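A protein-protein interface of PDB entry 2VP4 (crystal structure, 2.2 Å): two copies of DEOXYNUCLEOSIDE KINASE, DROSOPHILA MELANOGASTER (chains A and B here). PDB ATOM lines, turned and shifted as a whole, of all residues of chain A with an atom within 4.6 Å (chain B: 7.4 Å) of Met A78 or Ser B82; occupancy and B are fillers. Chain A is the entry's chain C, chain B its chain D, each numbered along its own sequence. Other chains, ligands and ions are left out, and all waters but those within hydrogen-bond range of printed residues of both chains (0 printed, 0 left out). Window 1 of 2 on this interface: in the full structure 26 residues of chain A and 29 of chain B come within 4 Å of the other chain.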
ATOM      1  N   TRP A  76       0.905 -33.243  27.704  1.00  0.00           N
ATOM      2  CA  TRP A  76       1.530 -33.625  26.420  1.00  0.00           C
ATOM      3  C   TRP A  76       0.691 -33.455  25.163  1.00  0.00           C
ATOM      4  O   TRP A  76       1.215 -33.566  24.048  1.00  0.00           O
ATOM      5  CB  TRP A  76       2.073 -35.052  26.482  1.00  0.00           C
ATOM      6  CG  TRP A  76       3.361 -35.151  27.231  1.00  0.00           C
ATOM      7  CD1 TRP A  76       3.523 -35.524  28.530  1.00  0.00           C
ATOM      8  CD2 TRP A  76       4.665 -34.854  26.729  1.00  0.00           C
ATOM      9  NE1 TRP A  76       4.852 -35.489  28.874  1.00  0.00           N
ATOM     10  CE2 TRP A  76       5.579 -35.079  27.787  1.00  0.00           C
ATOM     11  CE3 TRP A  76       5.154 -34.415  25.491  1.00  0.00           C
ATOM     12  CZ2 TRP A  76       6.956 -34.875  27.646  1.00  0.00           C
ATOM     13  CZ3 TRP A  76       6.527 -34.221  25.344  1.00  0.00           C
ATOM     14  CH2 TRP A  76       7.410 -34.451  26.418  1.00  0.00           C
ATOM     15  N   ALA A  77      -0.598 -33.195  25.341  1.00  0.00           N
ATOM     16  CA  ALA A  77      -1.520 -33.033  24.228  1.00  0.00           C
ATOM     17  C   ALA A  77      -1.197 -31.821  23.359  1.00  0.00           C
ATOM     18  O   ALA A  77      -1.392 -31.862  22.143  1.00  0.00           O
ATOM     19  CB  ALA A  77      -2.957 -32.944  24.734  1.00  0.00           C
ATOM     20  N   MET A  78      -0.714 -30.737  23.971  1.00  0.00           N
ATOM     21  CA  MET A  78      -0.406 -29.534  23.205  1.00  0.00           C
ATOM     22  C   MET A  78       0.881 -29.722  22.396  1.00  0.00           C
ATOM     23  O   MET A  78       0.906 -29.431  21.207  1.00  0.00           O
ATOM     24  CB  MET A  78      -0.399 -28.262  24.102  1.00  0.00           C
ATOM     25  CG  MET A  78      -0.300 -26.899  23.351  1.00  0.00           C
ATOM     26  SD  MET A  78       1.437 -26.568  23.029  1.00  0.00           S
ATOM     27  CE  MET A  78       1.389 -25.280  21.787  1.00  0.00           C
ATOM     28  N   PRO A  79       1.962 -30.202  23.025  1.00  0.00           N
ATOM     29  CA  PRO A  79       3.090 -30.476  22.117  1.00  0.00           C
ATOM     30  C   PRO A  79       2.825 -31.595  21.084  1.00  0.00           C
ATOM     31  O   PRO A  79       3.328 -31.517  19.980  1.00  0.00           O
ATOM     32  CB  PRO A  79       4.239 -30.855  23.068  1.00  0.00           C
ATOM     33  CG  PRO A  79       3.580 -31.263  24.353  1.00  0.00           C
ATOM     34  CD  PRO A  79       2.309 -30.438  24.442  1.00  0.00           C
ATOM     35  N   PHE A  80       2.044 -32.616  21.430  1.00  0.00           N
ATOM     36  CA  PHE A  80       1.659 -33.630  20.441  1.00  0.00           C
ATOM     37  C   PHE A  80       0.924 -33.001  19.244  1.00  0.00           C
ATOM     38  O   PHE A  80       1.323 -33.179  18.095  1.00  0.00           O
ATOM     39  CB  PHE A  80       0.808 -34.757  21.072  1.00  0.00           C
ATOM     40  CG  PHE A  80       0.268 -35.719  20.063  1.00  0.00           C
ATOM     41  CD1 PHE A  80       1.076 -36.731  19.553  1.00  0.00           C
ATOM     42  CD2 PHE A  80      -1.014 -35.566  19.568  1.00  0.00           C
ATOM     43  CE1 PHE A  80       0.598 -37.591  18.578  1.00  0.00           C
ATOM     44  CE2 PHE A  80      -1.505 -36.431  18.621  1.00  0.00           C
ATOM     45  CZ  PHE A  80      -0.696 -37.448  18.117  1.00  0.00           C
ATOM     46  N   GLN A  81      -0.126 -32.235  19.518  1.00  0.00           N
ATOM     47  CA  GLN A  81      -0.917 -31.631  18.443  1.00  0.00           C
ATOM     48  C   GLN A  81      -0.128 -30.564  17.680  1.00  0.00           C
ATOM     49  O   GLN A  81      -0.299 -30.375  16.465  1.00  0.00           O
ATOM     50  CB  GLN A  81      -2.204 -31.029  18.998  1.00  0.00           C
ATOM     51  CG  GLN A  81      -3.314 -32.029  19.375  1.00  0.00           C
ATOM     52  CD  GLN A  81      -3.675 -33.042  18.279  1.00  0.00           C
ATOM     53  OE1 GLN A  81      -3.918 -34.203  18.579  1.00  0.00           O
ATOM     54  NE2 GLN A  81      -3.737 -32.607  17.032  1.00  0.00           N
ATOM     55  N   SER A  82       0.733 -29.856  18.404  1.00  0.00           N
ATOM     56  CA  SER A  82       1.693 -28.956  17.758  1.00  0.00           C
ATOM     57  C   SER A  82       2.602 -29.720  16.781  1.00  0.00           C
ATOM     58  O   SER A  82       2.835 -29.302  15.638  1.00  0.00           O
ATOM     59  CB  SER A  82       2.515 -28.213  18.825  1.00  0.00           C
ATOM     60  OG  SER A  82       3.360 -27.293  18.181  1.00  0.00           O
ATOM     61  N   LEU A 124      -6.666 -30.304  26.750  1.00  0.00           N
ATOM     62  CA  LEU A 124      -6.066 -29.026  26.413  1.00  0.00           C
ATOM     63  C   LEU A 124      -6.788 -27.968  27.236  1.00  0.00           C
ATOM     64  O   LEU A 124      -8.000 -27.814  27.112  1.00  0.00           O
ATOM     65  CB  LEU A 124      -6.239 -28.722  24.918  1.00  0.00           C
ATOM     66  CG  LEU A 124      -5.506 -29.557  23.860  1.00  0.00           C
ATOM     67  CD1 LEU A 124      -6.029 -29.257  22.447  1.00  0.00           C
ATOM     68  CD2 LEU A 124      -4.005 -29.347  23.922  1.00  0.00           C
ATOM     69  N   MET A 128      -3.631 -23.513  26.225  1.00  0.00           N
ATOM     70  CA  MET A 128      -3.110 -24.397  25.176  1.00  0.00           C
ATOM     71  C   MET A 128      -3.960 -24.358  23.901  1.00  0.00           C
ATOM     72  O   MET A 128      -3.437 -24.215  22.791  1.00  0.00           O
ATOM     73  CB  MET A 128      -3.013 -25.816  25.720  1.00  0.00           C
ATOM     74  CG  MET A 128      -1.832 -26.000  26.638  1.00  0.00           C
ATOM     75  SD  MET A 128      -2.188 -27.223  27.881  1.00  0.00           S
ATOM     76  CE  MET A 128      -0.546 -27.410  28.604  1.00  0.00           C
ATOM     77  N   THR A 131      -3.428 -21.021  22.118  1.00  0.00           N
ATOM     78  CA  THR A 131      -2.125 -20.962  21.485  1.00  0.00           C
ATOM     79  C   THR A 131      -2.176 -21.734  20.162  1.00  0.00           C
ATOM     80  O   THR A 131      -1.589 -21.314  19.160  1.00  0.00           O
ATOM     81  CB  THR A 131      -1.014 -21.541  22.430  1.00  0.00           C
ATOM     82  OG1 THR A 131      -0.915 -20.747  23.613  1.00  0.00           O
ATOM     83  CG2 THR A 131       0.349 -21.570  21.767  1.00  0.00           C
ATOM     84  N   LEU A 132      -2.863 -22.875  20.169  1.00  0.00           N
ATOM     85  CA  LEU A 132      -3.025 -23.680  18.945  1.00  0.00           C
ATOM     86  C   LEU A 132      -3.855 -22.961  17.867  1.00  0.00           C
ATOM     87  O   LEU A 132      -3.432 -22.894  16.714  1.00  0.00           O
ATOM     88  CB  LEU A 132      -3.563 -25.090  19.265  1.00  0.00           C
ATOM     89  CG  LEU A 132      -2.589 -26.008  20.038  1.00  0.00           C
ATOM     90  CD1 LEU A 132      -3.243 -27.340  20.438  1.00  0.00           C
ATOM     91  CD2 LEU A 132      -1.227 -26.260  19.324  1.00  0.00           C
ATOM     92  N   TRP A 135      -2.042 -20.096  16.312  1.00  0.00           N
ATOM     93  CA  TRP A 135      -1.152 -20.719  15.319  1.00  0.00           C
ATOM     94  C   TRP A 135      -1.907 -21.080  14.026  1.00  0.00           C
ATOM     95  O   TRP A 135      -1.501 -20.678  12.921  1.00  0.00           O
ATOM     96  CB  TRP A 135      -0.398 -21.927  15.914  1.00  0.00           C
ATOM     97  CG  TRP A 135       1.024 -21.606  16.341  1.00  0.00           C
ATOM     98  CD1 TRP A 135       1.509 -21.572  17.618  1.00  0.00           C
ATOM     99  CD2 TRP A 135       2.131 -21.284  15.486  1.00  0.00           C
ATOM    100  NE1 TRP A 135       2.863 -21.236  17.620  1.00  0.00           N
ATOM    101  CE2 TRP A 135       3.264 -21.051  16.326  1.00  0.00           C
ATOM    102  CE3 TRP A 135       2.282 -21.160  14.096  1.00  0.00           C
ATOM    103  CZ2 TRP A 135       4.522 -20.713  15.814  1.00  0.00           C
ATOM    104  CZ3 TRP A 135       3.534 -20.823  13.589  1.00  0.00           C
ATOM    105  CH2 TRP A 135       4.638 -20.600  14.450  1.00  0.00           C
ATOM    106  N   LEU B  65      -0.272 -16.606  30.085  1.00  0.00           N
ATOM    107  CA  LEU B  65       0.697 -17.668  29.819  1.00  0.00           C
ATOM    108  C   LEU B  65       2.018 -17.444  30.545  1.00  0.00           C
ATOM    109  O   LEU B  65       2.622 -18.417  30.995  1.00  0.00           O
ATOM    110  CB  LEU B  65       0.936 -17.841  28.310  1.00  0.00           C
ATOM    111  CG  LEU B  65      -0.186 -18.444  27.455  1.00  0.00           C
ATOM    112  CD1 LEU B  65       0.236 -18.471  26.012  1.00  0.00           C
ATOM    113  CD2 LEU B  65      -0.569 -19.857  27.931  1.00  0.00           C
ATOM    114  N   LYS B  75       4.589 -27.971  32.517  1.00  0.00           N
ATOM    115  CA  LYS B  75       3.331 -28.030  31.769  1.00  0.00           C
ATOM    116  C   LYS B  75       3.179 -26.840  30.798  1.00  0.00           C
ATOM    117  O   LYS B  75       2.639 -26.983  29.686  1.00  0.00           O
ATOM    118  CB  LYS B  75       2.137 -28.059  32.738  1.00  0.00           C
ATOM    119  CG  LYS B  75       0.785 -28.331  32.105  1.00  0.00           C
ATOM    120  CD  LYS B  75      -0.352 -28.166  33.130  1.00  0.00           C
ATOM    121  CE  LYS B  75      -1.661 -28.757  32.625  1.00  0.00           C
ATOM    122  NZ  LYS B  75      -2.869 -28.288  33.388  1.00  0.00           N
ATOM    123  N   TRP B  76       3.648 -25.669  31.222  1.00  0.00           N
ATOM    124  CA  TRP B  76       3.291 -24.440  30.539  1.00  0.00           C
ATOM    125  C   TRP B  76       4.412 -23.744  29.764  1.00  0.00           C
ATOM    126  O   TRP B  76       4.134 -22.832  28.997  1.00  0.00           O
ATOM    127  CB  TRP B  76       2.556 -23.487  31.492  1.00  0.00           C
ATOM    128  CG  TRP B  76       1.143 -23.940  31.793  1.00  0.00           C
ATOM    129  CD1 TRP B  76       0.721 -24.657  32.883  1.00  0.00           C
ATOM    130  CD2 TRP B  76      -0.016 -23.738  30.976  1.00  0.00           C
ATOM    131  NE1 TRP B  76      -0.630 -24.902  32.797  1.00  0.00           N
ATOM    132  CE2 TRP B  76      -1.110 -24.348  31.639  1.00  0.00           C
ATOM    133  CE3 TRP B  76      -0.243 -23.102  29.744  1.00  0.00           C
ATOM    134  CZ2 TRP B  76      -2.412 -24.331  31.117  1.00  0.00           C
ATOM    135  CZ3 TRP B  76      -1.552 -23.086  29.223  1.00  0.00           C
ATOM    136  CH2 TRP B  76      -2.611 -23.686  29.913  1.00  0.00           C
ATOM    137  N   ALA B  77       5.652 -24.200  29.930  1.00  0.00           N
ATOM    138  CA  ALA B  77       6.793 -23.655  29.188  1.00  0.00           C
ATOM    139  C   ALA B  77       6.716 -23.892  27.677  1.00  0.00           C
ATOM    140  O   ALA B  77       7.023 -22.988  26.900  1.00  0.00           O
ATOM    141  CB  ALA B  77       8.120 -24.180  29.757  1.00  0.00           C
ATOM    142  N   MET B  78       6.285 -25.083  27.254  1.00  0.00           N
ATOM    143  CA  MET B  78       6.158 -25.383  25.808  1.00  0.00           C
ATOM    144  C   MET B  78       5.116 -24.492  25.134  1.00  0.00           C
ATOM    145  O   MET B  78       5.446 -23.831  24.150  1.00  0.00           O
ATOM    146  CB  MET B  78       5.910 -26.890  25.527  1.00  0.00           C
ATOM    147  CG  MET B  78       6.234 -27.370  24.073  1.00  0.00           C
ATOM    148  SD  MET B  78       4.853 -27.033  22.950  1.00  0.00           S
ATOM    149  CE  MET B  78       5.666 -27.288  21.371  1.00  0.00           C
ATOM    150  N   PRO B  79       3.861 -24.474  25.646  1.00  0.00           N
ATOM    151  CA  PRO B  79       2.870 -23.585  25.019  1.00  0.00           C
ATOM    152  C   PRO B  79       3.217 -22.097  25.098  1.00  0.00           C
ATOM    153  O   PRO B  79       2.883 -21.329  24.186  1.00  0.00           O
ATOM    154  CB  PRO B  79       1.562 -23.875  25.790  1.00  0.00           C
ATOM    155  CG  PRO B  79       1.941 -24.592  27.006  1.00  0.00           C
ATOM    156  CD  PRO B  79       3.271 -25.265  26.748  1.00  0.00           C
ATOM    157  N   PHE B  80       3.858 -21.691  26.192  1.00  0.00           N
ATOM    158  CA  PHE B  80       4.385 -20.340  26.294  1.00  0.00           C
ATOM    159  C   PHE B  80       5.371 -20.025  25.164  1.00  0.00           C
ATOM    160  O   PHE B  80       5.155 -19.060  24.420  1.00  0.00           O
ATOM    161  CB  PHE B  80       5.019 -20.085  27.680  1.00  0.00           C
ATOM    162  CG  PHE B  80       5.634 -18.725  27.812  1.00  0.00           C
ATOM    163  CD1 PHE B  80       4.831 -17.605  28.005  1.00  0.00           C
ATOM    164  CD2 PHE B  80       7.017 -18.558  27.691  1.00  0.00           C
ATOM    165  CE1 PHE B  80       5.398 -16.326  28.104  1.00  0.00           C
ATOM    166  CE2 PHE B  80       7.599 -17.284  27.801  1.00  0.00           C
ATOM    167  CZ  PHE B  80       6.786 -16.166  28.005  1.00  0.00           C
ATOM    168  N   GLN B  81       6.449 -20.813  25.025  1.00  0.00           N
ATOM    169  CA  GLN B  81       7.450 -20.482  24.000  1.00  0.00           C
ATOM    170  C   GLN B  81       6.837 -20.561  22.593  1.00  0.00           C
ATOM    171  O   GLN B  81       7.243 -19.854  21.669  1.00  0.00           O
ATOM    172  CB  GLN B  81       8.715 -21.371  24.078  1.00  0.00           C
ATOM    173  CG  GLN B  81       9.609 -21.139  25.299  1.00  0.00           C
ATOM    174  CD  GLN B  81      10.043 -19.674  25.514  1.00  0.00           C
ATOM    175  OE1 GLN B  81      10.346 -19.271  26.645  1.00  0.00           O
ATOM    176  NE2 GLN B  81      10.124 -18.897  24.431  1.00  0.00           N
ATOM    177  N   SER B  82       5.865 -21.452  22.440  1.00  0.00           N
ATOM    178  CA  SER B  82       5.190 -21.641  21.164  1.00  0.00           C
ATOM    179  C   SER B  82       4.352 -20.398  20.858  1.00  0.00           C
ATOM    180  O   SER B  82       4.315 -19.919  19.726  1.00  0.00           O
ATOM    181  CB  SER B  82       4.341 -22.913  21.227  1.00  0.00           C
ATOM    182  OG  SER B  82       3.685 -23.127  20.004  1.00  0.00           O
ATOM    183  N   TYR B  83       3.694 -19.845  21.867  1.00  0.00           N
ATOM    184  CA  TYR B  83       3.026 -18.569  21.654  1.00  0.00           C
ATOM    185  C   TYR B  83       4.003 -17.396  21.381  1.00  0.00           C
ATOM    186  O   TYR B  83       3.738 -16.556  20.515  1.00  0.00           O
ATOM    187  CB  TYR B  83       2.062 -18.257  22.777  1.00  0.00           C
ATOM    188  CG  TYR B  83       1.144 -17.107  22.449  1.00  0.00           C
ATOM    189  CD1 TYR B  83       0.149 -17.234  21.483  1.00  0.00           C
ATOM    190  CD2 TYR B  83       1.291 -15.870  23.093  1.00  0.00           C
ATOM    191  CE1 TYR B  83      -0.699 -16.161  21.169  1.00  0.00           C
ATOM    192  CE2 TYR B  83       0.464 -14.796  22.783  1.00  0.00           C
ATOM    193  CZ  TYR B  83      -0.535 -14.953  21.826  1.00  0.00           C
ATOM    194  OH  TYR B  83      -1.362 -13.892  21.530  1.00  0.00           O
ATOM    195  N   VAL B  84       5.145 -17.373  22.074  1.00  0.00           N
ATOM    196  CA  VAL B  84       6.146 -16.322  21.892  1.00  0.00           C
ATOM    197  C   VAL B  84       6.666 -16.342  20.472  1.00  0.00           C
ATOM    198  O   VAL B  84       6.789 -15.294  19.844  1.00  0.00           O
ATOM    199  CB  VAL B  84       7.372 -16.462  22.854  1.00  0.00           C
ATOM    200  CG1 VAL B  84       8.482 -15.496  22.454  1.00  0.00           C
ATOM    201  CG2 VAL B  84       6.972 -16.232  24.287  1.00  0.00           C
ATOM    202  N   THR B  85       6.996 -17.542  20.002  1.00  0.00           N
ATOM    203  CA  THR B  85       7.435 -17.774  18.623  1.00  0.00           C
ATOM    204  C   THR B  85       6.446 -17.199  17.631  1.00  0.00           C
ATOM    205  O   THR B  85       6.843 -16.529  16.685  1.00  0.00           O
ATOM    206  CB  THR B  85       7.665 -19.284  18.374  1.00  0.00           C
ATOM    207  OG1 THR B  85       8.628 -19.764  19.315  1.00  0.00           O
ATOM    208  CG2 THR B  85       8.158 -19.562  16.959  1.00  0.00           C
ATOM    209  N   LEU B  86       5.157 -17.426  17.878  1.00  0.00           N
ATOM    210  CA  LEU B  86       4.092 -16.925  17.015  1.00  0.00           C
ATOM    211  C   LEU B  86       4.055 -15.393  16.965  1.00  0.00           C
ATOM    212  O   LEU B  86       4.004 -14.788  15.878  1.00  0.00           O
ATOM    213  CB  LEU B  86       2.740 -17.462  17.493  1.00  0.00           C
ATOM    214  CG  LEU B  86       1.495 -16.947  16.754  1.00  0.00           C
ATOM    215  CD1 LEU B  86       1.603 -17.183  15.241  1.00  0.00           C
ATOM    216  CD2 LEU B  86       0.236 -17.523  17.300  1.00  0.00           C
ATOM    217  N   THR B  87       4.077 -14.771  18.144  1.00  0.00           N
ATOM    218  CA  THR B  87       3.983 -13.328  18.264  1.00  0.00           C
ATOM    219  C   THR B  87       5.154 -12.671  17.567  1.00  0.00           C
ATOM    220  O   THR B  87       4.983 -11.634  16.937  1.00  0.00           O
ATOM    221  CB  THR B  87       3.920 -12.865  19.735  1.00  0.00           C
ATOM    222  OG1 THR B  87       5.079 -13.332  20.431  1.00  0.00           O
ATOM    223  CG2 THR B  87       2.680 -13.385  20.409  1.00  0.00           C
ATOM    224  N   MET B  88       6.338 -13.277  17.665  1.00  0.00           N
ATOM    225  CA  MET B  88       7.526 -12.761  16.973  1.00  0.00           C
ATOM    226  C   MET B  88       7.356 -12.849  15.448  1.00  0.00           C
ATOM    227  O   MET B  88       7.619 -11.886  14.736  1.00  0.00           O
ATOM    228  CB  MET B  88       8.796 -13.510  17.413  1.00  0.00           C
ATOM    229  CG  MET B  88       9.146 -13.391  18.902  1.00  0.00           C
ATOM    230  SD  MET B  88       9.283 -11.664  19.466  1.00  0.00           S
ATOM    231  CE  MET B  88       7.599 -11.323  19.998  1.00  0.00           C
ATOM    232  N   LEU B  89       6.935 -14.019  14.968  1.00  0.00           N
ATOM    233  CA  LEU B  89       6.567 -14.237  13.556  1.00  0.00           C
ATOM    234  C   LEU B  89       5.475 -13.277  13.068  1.00  0.00           C
ATOM    235  O   LEU B  89       5.562 -12.746  11.983  1.00  0.00           O
ATOM    236  CB  LEU B  89       6.128 -15.689  13.342  1.00  0.00           C
ATOM    237  CG  LEU B  89       7.082 -16.655  12.637  1.00  0.00           C
ATOM    238  CD1 LEU B  89       8.557 -16.305  12.756  1.00  0.00           C
ATOM    239  CD2 LEU B  89       6.817 -18.045  13.152  1.00  0.00           C
ATOM    240  N   VAL B 115      14.310 -20.860  24.981  1.00  0.00           N
ATOM    241  CA  VAL B 115      14.047 -22.301  24.735  1.00  0.00           C
ATOM    242  C   VAL B 115      15.260 -23.168  25.117  1.00  0.00           C
ATOM    243  O   VAL B 115      15.116 -24.135  25.868  1.00  0.00           O
ATOM    244  CB  VAL B 115      13.620 -22.562  23.250  1.00  0.00           C
ATOM    245  CG1 VAL B 115      13.530 -24.096  22.931  1.00  0.00           C
ATOM    246  CG2 VAL B 115      12.307 -21.885  22.965  1.00  0.00           C
ATOM    247  N   MET B 128       9.322 -31.929  24.111  1.00  0.00           N
ATOM    248  CA  MET B 128       8.865 -30.544  23.949  1.00  0.00           C
ATOM    249  C   MET B 128       9.907 -29.709  23.185  1.00  0.00           C
ATOM    250  O   MET B 128       9.575 -29.043  22.210  1.00  0.00           O
ATOM    251  CB  MET B 128       8.573 -29.937  25.306  1.00  0.00           C
ATOM    252  CG  MET B 128       7.261 -30.391  25.880  1.00  0.00           C
ATOM    253  SD  MET B 128       7.354 -30.350  27.658  1.00  0.00           S
ATOM    254  CE  MET B 128       5.737 -31.008  28.064  1.00  0.00           C
ATOM    255  N   THR B 131      10.116 -30.731  19.504  1.00  0.00           N
ATOM    256  CA  THR B 131       8.967 -30.182  18.784  1.00  0.00           C
ATOM    257  C   THR B 131       9.211 -28.728  18.398  1.00  0.00           C
ATOM    258  O   THR B 131       8.949 -28.326  17.260  1.00  0.00           O
ATOM    259  CB  THR B 131       7.660 -30.330  19.618  1.00  0.00           C
ATOM    260  OG1 THR B 131       7.412 -31.724  19.858  1.00  0.00           O
ATOM    261  CG2 THR B 131       6.462 -29.740  18.899  1.00  0.00           C
ATOM    262  N   LEU B 132       9.729 -27.942  19.353  1.00  0.00           N
ATOM    263  CA  LEU B 132      10.090 -26.547  19.104  1.00  0.00           C
ATOM    264  C   LEU B 132      11.180 -26.421  18.072  1.00  0.00           C
ATOM    265  O   LEU B 132      11.042 -25.616  17.129  1.00  0.00           O
ATOM    266  CB  LEU B 132      10.487 -25.843  20.405  1.00  0.00           C
ATOM    267  CG  LEU B 132       9.304 -25.796  21.369  1.00  0.00           C
ATOM    268  CD1 LEU B 132       9.768 -25.652  22.798  1.00  0.00           C
ATOM    269  CD2 LEU B 132       8.309 -24.718  21.016  1.00  0.00           C
ATOM    270  N   TRP B 135       9.827 -27.194  14.671  1.00  0.00           N
ATOM    271  CA  TRP B 135       9.114 -25.993  14.225  1.00  0.00           C
ATOM    272  C   TRP B 135      10.050 -24.884  13.709  1.00  0.00           C
ATOM    273  O   TRP B 135       9.827 -24.321  12.654  1.00  0.00           O
ATOM    274  CB  TRP B 135       8.201 -25.460  15.321  1.00  0.00           C
ATOM    275  CG  TRP B 135       6.798 -25.911  15.162  1.00  0.00           C
ATOM    276  CD1 TRP B 135       6.158 -26.901  15.875  1.00  0.00           C
ATOM    277  CD2 TRP B 135       5.840 -25.415  14.219  1.00  0.00           C
ATOM    278  NE1 TRP B 135       4.865 -27.045  15.429  1.00  0.00           N
ATOM    279  CE2 TRP B 135       4.639 -26.143  14.420  1.00  0.00           C
ATOM    280  CE3 TRP B 135       5.877 -24.429  13.223  1.00  0.00           C
ATOM    281  CZ2 TRP B 135       3.474 -25.900  13.660  1.00  0.00           C
ATOM    282  CZ3 TRP B 135       4.720 -24.194  12.467  1.00  0.00           C
ATOM    283  CH2 TRP B 135       3.535 -24.925  12.702  1.00  0.00           C
ATOM    284  N   TYR B 136      11.117 -24.614  14.454  1.00  0.00           N
ATOM    285  CA  TYR B 136      12.113 -23.604  14.065  1.00  0.00           C
ATOM    286  C   TYR B 136      12.741 -23.877  12.700  1.00  0.00           C
ATOM    287  O   TYR B 136      12.949 -22.957  11.923  1.00  0.00           O
ATOM    288  CB  TYR B 136      13.198 -23.461  15.156  1.00  0.00           C
ATOM    289  CG  TYR B 136      12.705 -22.731  16.397  1.00  0.00           C
ATOM    290  CD1 TYR B 136      12.942 -23.240  17.688  1.00  0.00           C
ATOM    291  CD2 TYR B 136      11.975 -21.552  16.280  1.00  0.00           C
ATOM    292  CE1 TYR B 136      12.471 -22.572  18.822  1.00  0.00           C
ATOM    293  CE2 TYR B 136      11.507 -20.886  17.380  1.00  0.00           C
ATOM    294  CZ  TYR B 136      11.759 -21.384  18.647  1.00  0.00           C
ATOM    295  OH  TYR B 136      11.272 -20.686  19.726  1.00  0.00           O
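Printed residues of chain B that touch a printed residue of chain A: Leu B65, Lys B75, Trp B76, Met B78, Pro B79, Ser B82, Tyr B83, Thr B85, Leu B86, Leu B89, Met B128, Thr B131 and Trp B135. Hydrophobic or aromatic side chains of chain B within 4 Å of the printed part of chain A: Leu B65, Trp B76, Met B78, Pro B79, Tyr B83, Leu B86, Leu B89, Met B128 and Trp B135. Of the 12 printed residues of chain A, 7 touch a printed residue of chain B. Hydrophobic or aromatic side chains of chain A within 4 Å of the printed part of chain B: Trp A76, Met A78, Pro A79, Met A128 and Trp A135. Among the printed residues, 18 pairs touch across the chains.
Trp A76 touches Met B128 (CZ3 to N, 3.8 Å). Met A78 touches Pro B79 (SD to CB, 3.9 Å). CE of Met A78 touches OG of Ser B82, at 3.6 Å. Met B78 touches Pro A79. Thr B131 touches Pro A79 (CG2 to O, 3.8 Å). CD1 of Leu B65 touches OG1 of Thr A131 (3.5 Å). O of Pro B79 touches CG2 of Thr A131, at 3.5 Å. Thr A131 touches Tyr B83 (CG2 to N, 3.8 Å). Trp A135 touches Thr B85 (CZ2 to CG2, 3.98 Å). CZ3 of Trp A135 touches CZ3 of Trp B135, at 3.7 Å.
No residue of chain B comes within 4 Å of Ala A77. Of the printed residues of chain B, Met A78 touches Met B78, Pro B79 and Ser B82. Leu A124 touches none of the printed residues of chain B. Of the printed residues of chain B, Trp A135 touches Ser B82, Thr B85, Leu B86, Leu B89 and Trp B135. Of the printed residues of chain A, Leu B65 touches Thr A131. Gln B81 touches none of the printed residues of chain A. Printed residues of chain A within 4 Å of Thr B85: Trp A135 (3.98 Å). Of the printed residues of chain A, Leu B89 touches Trp A135. Printed residues of chain A within 4 Å of Thr B131: Pro A79. The nearest residue of chain B that does not touch Met A78 is Tyr B83 (5.9 Å). The nearest residue of chain A that does not touch Ser B82 is Thr A131 (4.1 Å). The nearest printed residue of chain B that does not touch Trp A135 is Tyr B83 (4.5 Å).
NE1 of Trp B135 is in hydrogen-bond range of O of Ser A82, at 3.0 Å. The backbone carbonyl oxygen (O) of Ser B82 is in hydrogen-bond range of the indole nitrogen (NE1) of Trp A135, 2.9 Å away. The side-chain sulfur (SD) of Met B78 lies close to the side-chain sulfur (SD) of Met A78, 3.4 Å away.
Trp A76 touches Met B128, and with the chains exchanged Met A128 touches Trp B76. Met A78 touches Ser B82, and with the chains exchanged Ser A82 touches Met B78. Pro A79 touches Thr B131, and with the chains exchanged Thr A131 touches Pro B79. Trp B135 touches its own counterpart, Trp A135. 11 positions are printed for both chains. Of the 18 pairs that touch across the chains among the printed residues, 12 have their exchanged pair printed and touching as well.
OG1 of Thr B85 is in hydrogen-bond range of O of Gln B81. The backbone carbonyl oxygen (O) of Tyr B83 lies close to the side-chain hydroxyl (OG1) of Thr B87 (3.5 Å). The side-chain hydroxyl of Thr B85 lies within hydrogen-bond range of the side-chain hydroxyl of Tyr B136 (2.8 Å).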
